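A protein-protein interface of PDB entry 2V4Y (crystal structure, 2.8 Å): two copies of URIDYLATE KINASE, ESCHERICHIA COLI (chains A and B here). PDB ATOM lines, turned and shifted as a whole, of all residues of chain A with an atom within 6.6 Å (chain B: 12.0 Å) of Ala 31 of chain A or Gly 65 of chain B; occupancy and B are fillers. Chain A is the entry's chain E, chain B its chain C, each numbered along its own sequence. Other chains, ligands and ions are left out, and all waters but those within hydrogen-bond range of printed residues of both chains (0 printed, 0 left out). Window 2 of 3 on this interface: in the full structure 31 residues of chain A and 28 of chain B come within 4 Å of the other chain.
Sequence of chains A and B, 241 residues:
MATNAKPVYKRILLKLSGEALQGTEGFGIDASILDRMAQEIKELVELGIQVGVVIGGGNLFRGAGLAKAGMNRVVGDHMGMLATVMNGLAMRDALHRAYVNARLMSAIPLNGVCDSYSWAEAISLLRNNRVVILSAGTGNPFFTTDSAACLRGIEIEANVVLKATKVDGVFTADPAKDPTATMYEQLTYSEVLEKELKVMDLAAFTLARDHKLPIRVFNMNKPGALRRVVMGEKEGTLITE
No position is printed for both chains.
O of Leu 66 of chain B sits at hydrogen-bond distance from N of Met 71 of chain B. OD2 of Asp 35 of chain A lies within salt-bridge range of NH1 of Arg 97 of chain A (3.0 Å).
Among the printed residues, merely in contact across the chains: Arg 97 of chain A with Gly 70 of chain B, Ala 31 of chain A with Ala 69 of chain B, Ile 29 of chain A with Met 79 of chain B, Ala 31 of chain A with Gly 65 of chain B, Leu 34 of chain A with Leu 66 of chain B, Arg 97 of chain A with Met 71 of chain B, Ala 31 of chain A with Leu 66 of chain B, Ile 29 of chain A with Leu 66 of chain B and Asp 35 of chain A with Ala 69 of chain B.
Ile 29 of chain A touches two residues of chain B. No residue of chain B comes within 4 Å of Asp 30 of chain A. Of chain B, only Gly 65 (3.6 Å), Leu 66 (3.7 Å) and Ala 69 (3.3 Å) come within 4 Å of Ala 31 of chain A. Ile 33 of chain A touches none of the printed residues of chain B. Of chain B, only Leu 66 (3.7 Å) comes within 4 Å of Leu 34 of chain A. Asp 35 of chain A touches just one residue of chain B: Ala 69 (3.8 Å). Of the printed residues of chain B, Arg 97 of chain A touches Ala 69 (3.1 Å), Gly 70 (3.0 Å) and Met 71 (3.7 Å). Of chain A, only Ala 31 (3.6 Å) comes within 4 Å of Gly 65 of chain B. Of the printed residues of chain A, Leu 66 of chain B touches Ile 29, Ala 31 and Leu 34. Printed residues of chain A within 4 Å of Ala 69 of chain B: Ala 31 (3.3 Å), Asp 35 (3.8 Å) and Arg 97 (3.1 Å). Of the printed residues of chain A, Gly 70 of chain B touches Arg 97. Of the printed residues of chain A, Met 79 of chain B touches Ile 29. The nearest residue of chain B that does not touch Ala 31 of chain A is Lys 68 of chain B (6.1 Å). The nearest printed residue of chain A that does not touch Met 71 of chain B is Leu 34 of chain A (5.2 Å).
NH1 of Arg 97 of chain A is in hydrogen-bond range of O of Ala 69 of chain B, 3.1 Å away.
Of the 11 printed residues of chain A, 5 touch a printed residue of chain B. Printed residues of chain A that touch a printed residue of chain B: Ile 29, Ala 31, Leu 34, Asp 35 and Arg 97. Of the 19 printed residues of chain B, 6 touch a printed residue of chain A. Printed residues of chain B that touch a printed residue of chain A: Gly 65, Leu 66, Ala 69, Gly 70, Met 71 and Met 79. Hydrophobic or aromatic side chains of chain B within 4 Å of the printed part of chain A: Leu 66, Ala 69 and Met 79. Among the printed residues, 10 pairs touch across the chains. Among the printed residues, no Asp or Glu carboxylate lies within 4 Å of a Lys or Arg side-chain nitrogen of the other chain.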
ATOM      1  N   LEU A  21     -22.080 -34.353   9.586  1.00  0.00           N
ATOM      2  CA  LEU A  21     -22.869 -33.573   8.637  1.00  0.00           C
ATOM      3  C   LEU A  21     -24.349 -33.964   8.656  1.00  0.00           C
ATOM      4  O   LEU A  21     -25.165 -33.385   7.927  1.00  0.00           O
ATOM      5  CB  LEU A  21     -22.291 -33.707   7.224  1.00  0.00           C
ATOM      6  CG  LEU A  21     -20.788 -33.486   7.040  1.00  0.00           C
ATOM      7  CD1 LEU A  21     -20.424 -33.489   5.573  1.00  0.00           C
ATOM      8  CD2 LEU A  21     -20.347 -32.187   7.679  1.00  0.00           C
ATOM      9  N   ILE A  29     -27.029 -35.237   4.465  1.00  0.00           N
ATOM     10  CA  ILE A  29     -26.291 -34.015   4.704  1.00  0.00           C
ATOM     11  C   ILE A  29     -27.279 -32.886   4.965  1.00  0.00           C
ATOM     12  O   ILE A  29     -28.129 -32.578   4.125  1.00  0.00           O
ATOM     13  CB  ILE A  29     -25.390 -33.668   3.494  1.00  0.00           C
ATOM     14  CG1 ILE A  29     -24.369 -34.787   3.241  1.00  0.00           C
ATOM     15  CG2 ILE A  29     -24.706 -32.323   3.692  1.00  0.00           C
ATOM     16  CD1 ILE A  29     -23.627 -34.662   1.908  1.00  0.00           C
ATOM     17  N   ASP A  30     -27.180 -32.279   6.140  1.00  0.00           N
ATOM     18  CA  ASP A  30     -28.020 -31.139   6.464  1.00  0.00           C
ATOM     19  C   ASP A  30     -27.354 -29.828   6.053  1.00  0.00           C
ATOM     20  O   ASP A  30     -26.315 -29.461   6.585  1.00  0.00           O
ATOM     21  CB  ASP A  30     -28.338 -31.124   7.956  1.00  0.00           C
ATOM     22  CG  ASP A  30     -29.089 -29.864   8.382  1.00  0.00           C
ATOM     23  OD1 ASP A  30     -30.039 -29.446   7.678  1.00  0.00           O
ATOM     24  OD2 ASP A  30     -28.723 -29.284   9.426  1.00  0.00           O
ATOM     25  N   ALA A  31     -27.962 -29.122   5.108  1.00  0.00           N
ATOM     26  CA  ALA A  31     -27.373 -27.900   4.557  1.00  0.00           C
ATOM     27  C   ALA A  31     -26.871 -26.925   5.621  1.00  0.00           C
ATOM     28  O   ALA A  31     -25.770 -26.393   5.514  1.00  0.00           O
ATOM     29  CB  ALA A  31     -28.356 -27.203   3.626  1.00  0.00           C
ATOM     30  N   SER A  32     -27.678 -26.688   6.648  1.00  0.00           N
ATOM     31  CA  SER A  32     -27.345 -25.693   7.662  1.00  0.00           C
ATOM     32  C   SER A  32     -26.216 -26.148   8.586  1.00  0.00           C
ATOM     33  O   SER A  32     -25.337 -25.369   8.932  1.00  0.00           O
ATOM     34  CB  SER A  32     -28.594 -25.327   8.463  1.00  0.00           C
ATOM     35  OG  SER A  32     -29.471 -26.436   8.553  1.00  0.00           O
ATOM     36  N   ILE A  33     -26.253 -27.409   8.987  1.00  0.00           N
ATOM     37  CA  ILE A  33     -25.207 -27.978   9.827  1.00  0.00           C
ATOM     38  C   ILE A  33     -23.893 -28.024   9.043  1.00  0.00           C
ATOM     39  O   ILE A  33     -22.811 -28.061   9.622  1.00  0.00           O
ATOM     40  CB  ILE A  33     -25.600 -29.400  10.313  1.00  0.00           C
ATOM     41  CG1 ILE A  33     -25.097 -29.669  11.725  1.00  0.00           C
ATOM     42  CG2 ILE A  33     -25.080 -30.463   9.355  1.00  0.00           C
ATOM     43  CD1 ILE A  33     -23.641 -30.095  11.779  1.00  0.00           C
ATOM     44  N   LEU A  34     -23.999 -28.011   7.719  1.00  0.00           N
ATOM     45  CA  LEU A  34     -22.834 -28.059   6.844  1.00  0.00           C
ATOM     46  C   LEU A  34     -22.255 -26.660   6.631  1.00  0.00           C
ATOM     47  O   LEU A  34     -21.048 -26.458   6.729  1.00  0.00           O
ATOM     48  CB  LEU A  34     -23.223 -28.662   5.491  1.00  0.00           C
ATOM     49  CG  LEU A  34     -22.128 -28.748   4.431  1.00  0.00           C
ATOM     50  CD1 LEU A  34     -21.240 -29.950   4.705  1.00  0.00           C
ATOM     51  CD2 LEU A  34     -22.739 -28.831   3.058  1.00  0.00           C
ATOM     52  N   ASP A  35     -23.124 -25.702   6.323  1.00  0.00           N
ATOM     53  CA  ASP A  35     -22.714 -24.316   6.157  1.00  0.00           C
ATOM     54  C   ASP A  35     -22.162 -23.752   7.456  1.00  0.00           C
ATOM     55  O   ASP A  35     -21.334 -22.847   7.454  1.00  0.00           O
ATOM     56  CB  ASP A  35     -23.892 -23.471   5.683  1.00  0.00           C
ATOM     57  CG  ASP A  35     -24.109 -23.563   4.190  1.00  0.00           C
ATOM     58  OD1 ASP A  35     -25.269 -23.688   3.753  1.00  0.00           O
ATOM     59  OD2 ASP A  35     -23.111 -23.502   3.445  1.00  0.00           O
ATOM     60  N   ARG A  36     -22.554 -24.287   8.583  1.00  0.00           N
ATOM     61  CA  ARG A  36     -21.935 -23.773   9.770  1.00  0.00           C
ATOM     62  C   ARG A  36     -20.568 -24.349   9.882  1.00  0.00           C
ATOM     63  O   ARG A  36     -19.664 -23.704  10.326  1.00  0.00           O
ATOM     64  CB  ARG A  36     -22.731 -24.070  11.028  1.00  0.00           C
ATOM     65  CG  ARG A  36     -22.399 -23.116  12.184  1.00  0.00           C
ATOM     66  CD  ARG A  36     -23.127 -21.787  12.049  1.00  0.00           C
ATOM     67  NE  ARG A  36     -22.224 -20.656  11.912  1.00  0.00           N
ATOM     68  CZ  ARG A  36     -21.061 -20.565  12.527  1.00  0.00           C
ATOM     69  NH1 ARG A  36     -20.662 -21.543  13.315  1.00  0.00           N
ATOM     70  NH2 ARG A  36     -20.295 -19.510  12.346  1.00  0.00           N
ATOM     71  N   ALA A  94     -19.799 -26.105  -0.151  1.00  0.00           N
ATOM     72  CA  ALA A  94     -20.154 -25.267   0.995  1.00  0.00           C
ATOM     73  C   ALA A  94     -19.126 -24.171   1.268  1.00  0.00           C
ATOM     74  O   ALA A  94     -19.488 -23.044   1.604  1.00  0.00           O
ATOM     75  CB  ALA A  94     -20.362 -26.117   2.241  1.00  0.00           C
ATOM     76  N   ARG A  97     -19.197 -21.335  -1.314  1.00  0.00           N
ATOM     77  CA  ARG A  97     -20.344 -20.482  -1.070  1.00  0.00           C
ATOM     78  C   ARG A  97     -20.075 -19.574   0.127  1.00  0.00           C
ATOM     79  O   ARG A  97     -20.736 -18.556   0.297  1.00  0.00           O
ATOM     80  CB  ARG A  97     -21.600 -21.329  -0.868  1.00  0.00           C
ATOM     81  CG  ARG A  97     -22.111 -21.989  -2.153  1.00  0.00           C
ATOM     82  CD  ARG A  97     -23.466 -22.675  -1.939  1.00  0.00           C
ATOM     83  NE  ARG A  97     -23.385 -23.871  -1.102  1.00  0.00           N
ATOM     84  CZ  ARG A  97     -23.722 -23.907   0.178  1.00  0.00           C
ATOM     85  NH1 ARG A  97     -24.168 -22.808   0.773  1.00  0.00           N
ATOM     86  NH2 ARG A  97     -23.610 -25.038   0.862  1.00  0.00           N
ATOM     87  N   GLY B  58     -31.143 -41.809  -5.991  1.00  0.00           N
ATOM     88  CA  GLY B  58     -32.076 -41.072  -5.153  1.00  0.00           C
ATOM     89  C   GLY B  58     -32.177 -41.543  -3.713  1.00  0.00           C
ATOM     90  O   GLY B  58     -32.471 -40.761  -2.817  1.00  0.00           O
ATOM     91  N   LEU B  60     -29.761 -42.612  -1.916  1.00  0.00           N
ATOM     92  CA  LEU B  60     -28.527 -42.319  -1.198  1.00  0.00           C
ATOM     93  C   LEU B  60     -28.198 -40.834  -1.222  1.00  0.00           C
ATOM     94  O   LEU B  60     -27.464 -40.336  -0.370  1.00  0.00           O
ATOM     95  CB  LEU B  60     -27.369 -43.130  -1.775  1.00  0.00           C
ATOM     96  CG  LEU B  60     -27.323 -44.583  -1.294  1.00  0.00           C
ATOM     97  CD1 LEU B  60     -26.281 -45.385  -2.073  1.00  0.00           C
ATOM     98  CD2 LEU B  60     -27.055 -44.637   0.203  1.00  0.00           C
ATOM     99  N   PHE B  61     -28.745 -40.125  -2.200  1.00  0.00           N
ATOM    100  CA  PHE B  61     -28.561 -38.689  -2.263  1.00  0.00           C
ATOM    101  C   PHE B  61     -29.829 -37.949  -2.675  1.00  0.00           C
ATOM    102  O   PHE B  61     -30.290 -38.054  -3.816  1.00  0.00           O
ATOM    103  CB  PHE B  61     -27.417 -38.330  -3.207  1.00  0.00           C
ATOM    104  CG  PHE B  61     -27.229 -36.849  -3.377  1.00  0.00           C
ATOM    105  CD1 PHE B  61     -26.699 -36.086  -2.347  1.00  0.00           C
ATOM    106  CD2 PHE B  61     -27.604 -36.220  -4.560  1.00  0.00           C
ATOM    107  CE1 PHE B  61     -26.538 -34.736  -2.496  1.00  0.00           C
ATOM    108  CE2 PHE B  61     -27.447 -34.864  -4.717  1.00  0.00           C
ATOM    109  CZ  PHE B  61     -26.910 -34.116  -3.682  1.00  0.00           C
ATOM    110  N   ARG B  62     -30.377 -37.187  -1.736  1.00  0.00           N
ATOM    111  CA  ARG B  62     -31.521 -36.333  -2.011  1.00  0.00           C
ATOM    112  C   ARG B  62     -31.003 -34.987  -2.499  1.00  0.00           C
ATOM    113  O   ARG B  62     -31.089 -34.659  -3.688  1.00  0.00           O
ATOM    114  CB  ARG B  62     -32.347 -36.137  -0.740  1.00  0.00           C
ATOM    115  CG  ARG B  62     -32.493 -37.394   0.112  1.00  0.00           C
ATOM    116  CD  ARG B  62     -33.485 -38.383  -0.499  1.00  0.00           C
ATOM    117  NE  ARG B  62     -34.009 -39.356   0.466  1.00  0.00           N
ATOM    118  CZ  ARG B  62     -34.198 -39.130   1.767  1.00  0.00           C
ATOM    119  NH1 ARG B  62     -34.684 -40.092   2.534  1.00  0.00           N
ATOM    120  NH2 ARG B  62     -33.923 -37.950   2.310  1.00  0.00           N
ATOM    121  N   GLY B  63     -30.459 -34.215  -1.565  1.00  0.00           N
ATOM    122  CA  GLY B  63     -29.791 -32.971  -1.897  1.00  0.00           C
ATOM    123  C   GLY B  63     -30.708 -31.900  -2.450  1.00  0.00           C
ATOM    124  O   GLY B  63     -30.274 -30.979  -3.142  1.00  0.00           O
ATOM    125  N   ALA B  64     -31.993 -32.021  -2.158  1.00  0.00           N
ATOM    126  CA  ALA B  64     -32.913 -30.953  -2.493  1.00  0.00           C
ATOM    127  C   ALA B  64     -32.676 -29.837  -1.481  1.00  0.00           C
ATOM    128  O   ALA B  64     -32.755 -28.651  -1.810  1.00  0.00           O
ATOM    129  CB  ALA B  64     -34.335 -31.450  -2.439  1.00  0.00           C
ATOM    130  N   GLY B  65     -32.360 -30.237  -0.251  1.00  0.00           N
ATOM    131  CA  GLY B  65     -32.036 -29.297   0.806  1.00  0.00           C
ATOM    132  C   GLY B  65     -30.742 -28.539   0.551  1.00  0.00           C
ATOM    133  O   GLY B  65     -30.648 -27.337   0.815  1.00  0.00           O
ATOM    134  N   LEU B  66     -29.738 -29.247   0.037  1.00  0.00           N
ATOM    135  CA  LEU B  66     -28.460 -28.628  -0.300  1.00  0.00           C
ATOM    136  C   LEU B  66     -28.588 -27.705  -1.511  1.00  0.00           C
ATOM    137  O   LEU B  66     -27.917 -26.679  -1.593  1.00  0.00           O
ATOM    138  CB  LEU B  66     -27.391 -29.692  -0.549  1.00  0.00           C
ATOM    139  CG  LEU B  66     -26.927 -30.446   0.697  1.00  0.00           C
ATOM    140  CD1 LEU B  66     -26.253 -31.756   0.319  1.00  0.00           C
ATOM    141  CD2 LEU B  66     -26.002 -29.576   1.533  1.00  0.00           C
ATOM    142  N   ALA B  67     -29.447 -28.072  -2.456  1.00  0.00           N
ATOM    143  CA  ALA B  67     -29.717 -27.206  -3.590  1.00  0.00           C
ATOM    144  C   ALA B  67     -30.377 -25.927  -3.078  1.00  0.00           C
ATOM    145  O   ALA B  67     -30.028 -24.820  -3.495  1.00  0.00           O
ATOM    146  CB  ALA B  67     -30.605 -27.908  -4.586  1.00  0.00           C
ATOM    147  N   LYS B  68     -31.326 -26.091  -2.159  1.00  0.00           N
ATOM    148  CA  LYS B  68     -32.002 -24.966  -1.526  1.00  0.00           C
ATOM    149  C   LYS B  68     -30.995 -24.027  -0.852  1.00  0.00           C
ATOM    150  O   LYS B  68     -31.138 -22.807  -0.910  1.00  0.00           O
ATOM    151  CB  LYS B  68     -33.029 -25.475  -0.507  1.00  0.00           C
ATOM    152  CG  LYS B  68     -33.932 -24.394   0.078  1.00  0.00           C
ATOM    153  CD  LYS B  68     -34.760 -24.903   1.268  1.00  0.00           C
ATOM    154  CE  LYS B  68     -36.027 -25.650   0.832  1.00  0.00           C
ATOM    155  NZ  LYS B  68     -35.836 -27.116   0.597  1.00  0.00           N
ATOM    156  N   ALA B  69     -29.975 -24.601  -0.220  1.00  0.00           N
ATOM    157  CA  ALA B  69     -28.954 -23.811   0.460  1.00  0.00           C
ATOM    158  C   ALA B  69     -27.983 -23.162  -0.520  1.00  0.00           C
ATOM    159  O   ALA B  69     -27.089 -22.428  -0.112  1.00  0.00           O
ATOM    160  CB  ALA B  69     -28.200 -24.669   1.463  1.00  0.00           C
ATOM    161  N   GLY B  70     -28.149 -23.443  -1.809  1.00  0.00           N
ATOM    162  CA  GLY B  70     -27.354 -22.795  -2.838  1.00  0.00           C
ATOM    163  C   GLY B  70     -26.248 -23.639  -3.449  1.00  0.00           C
ATOM    164  O   GLY B  70     -25.402 -23.123  -4.166  1.00  0.00           O
ATOM    165  N   MET B  71     -26.246 -24.936  -3.173  1.00  0.00           N
ATOM    166  CA  MET B  71     -25.214 -25.820  -3.712  1.00  0.00           C
ATOM    167  C   MET B  71     -25.203 -25.787  -5.219  1.00  0.00           C
ATOM    168  O   MET B  71     -26.258 -25.787  -5.846  1.00  0.00           O
ATOM    169  CB  MET B  71     -25.420 -27.259  -3.252  1.00  0.00           C
ATOM    170  CG  MET B  71     -24.667 -28.278  -4.084  1.00  0.00           C
ATOM    171  SD  MET B  71     -24.659 -29.934  -3.372  1.00  0.00           S
ATOM    172  CE  MET B  71     -23.568 -29.720  -1.976  1.00  0.00           C
ATOM    173  N   ASN B  72     -24.005 -25.765  -5.794  1.00  0.00           N
ATOM    174  CA  ASN B  72     -23.849 -25.732  -7.242  1.00  0.00           C
ATOM    175  C   ASN B  72     -24.503 -26.950  -7.889  1.00  0.00           C
ATOM    176  O   ASN B  72     -24.348 -28.082  -7.428  1.00  0.00           O
ATOM    177  CB  ASN B  72     -22.367 -25.625  -7.621  1.00  0.00           C
ATOM    178  CG  ASN B  72     -22.148 -25.623  -9.117  1.00  0.00           C
ATOM    179  OD1 ASN B  72     -22.233 -26.662  -9.759  1.00  0.00           O
ATOM    180  ND2 ASN B  72     -21.855 -24.457  -9.677  1.00  0.00           N
ATOM    181  N   ARG B  73     -25.245 -26.712  -8.959  1.00  0.00           N
ATOM    182  CA  ARG B  73     -25.985 -27.781  -9.613  1.00  0.00           C
ATOM    183  C   ARG B  73     -25.078 -28.935 -10.063  1.00  0.00           C
ATOM    184  O   ARG B  73     -25.413 -30.101  -9.889  1.00  0.00           O
ATOM    185  CB  ARG B  73     -26.778 -27.220 -10.798  1.00  0.00           C
ATOM    186  CG  ARG B  73     -28.077 -27.946 -11.069  1.00  0.00           C
ATOM    187  CD  ARG B  73     -28.982 -27.918  -9.846  1.00  0.00           C
ATOM    188  NE  ARG B  73     -30.072 -28.882  -9.965  1.00  0.00           N
ATOM    189  CZ  ARG B  73     -29.906 -30.200  -9.916  1.00  0.00           C
ATOM    190  NH1 ARG B  73     -28.686 -30.705  -9.755  1.00  0.00           N
ATOM    191  NH2 ARG B  73     -30.956 -31.010 -10.031  1.00  0.00           N
ATOM    192  N   VAL B  75     -22.020 -29.857  -8.901  1.00  0.00           N
ATOM    193  CA  VAL B  75     -21.565 -30.588  -7.731  1.00  0.00           C
ATOM    194  C   VAL B  75     -22.657 -31.513  -7.222  1.00  0.00           C
ATOM    195  O   VAL B  75     -22.389 -32.647  -6.827  1.00  0.00           O
ATOM    196  CB  VAL B  75     -21.129 -29.636  -6.600  1.00  0.00           C
ATOM    197  CG1 VAL B  75     -20.798 -30.416  -5.341  1.00  0.00           C
ATOM    198  CG2 VAL B  75     -19.926 -28.819  -7.041  1.00  0.00           C
ATOM    199  N   GLY B  76     -23.893 -31.021  -7.231  1.00  0.00           N
ATOM    200  CA  GLY B  76     -25.032 -31.813  -6.799  1.00  0.00           C
ATOM    201  C   GLY B  76     -25.185 -33.080  -7.612  1.00  0.00           C
ATOM    202  O   GLY B  76     -25.272 -34.176  -7.069  1.00  0.00           O
ATOM    203  N   ASP B  77     -25.206 -32.933  -8.927  1.00  0.00           N
ATOM    204  CA  ASP B  77     -25.305 -34.084  -9.803  1.00  0.00           C
ATOM    205  C   ASP B  77     -24.096 -35.022  -9.708  1.00  0.00           C
ATOM    206  O   ASP B  77     -24.236 -36.230  -9.878  1.00  0.00           O
ATOM    207  CB  ASP B  77     -25.564 -33.643 -11.243  1.00  0.00           C
ATOM    208  CG  ASP B  77     -27.009 -33.277 -11.472  1.00  0.00           C
ATOM    209  OD1 ASP B  77     -27.779 -33.368 -10.497  1.00  0.00           O
ATOM    210  OD2 ASP B  77     -27.380 -32.906 -12.607  1.00  0.00           O
ATOM    211  N   MET B  79     -22.575 -35.663  -6.992  1.00  0.00           N
ATOM    212  CA  MET B  79     -22.812 -36.427  -5.776  1.00  0.00           C
ATOM    213  C   MET B  79     -23.775 -37.559  -6.084  1.00  0.00           C
ATOM    214  O   MET B  79     -23.585 -38.692  -5.636  1.00  0.00           O
ATOM    215  CB  MET B  79     -23.364 -35.535  -4.676  1.00  0.00           C
ATOM    216  CG  MET B  79     -22.364 -34.542  -4.143  1.00  0.00           C
ATOM    217  SD  MET B  79     -23.015 -33.628  -2.754  1.00  0.00           S
ATOM    218  CE  MET B  79     -23.289 -34.924  -1.563  1.00  0.00           C
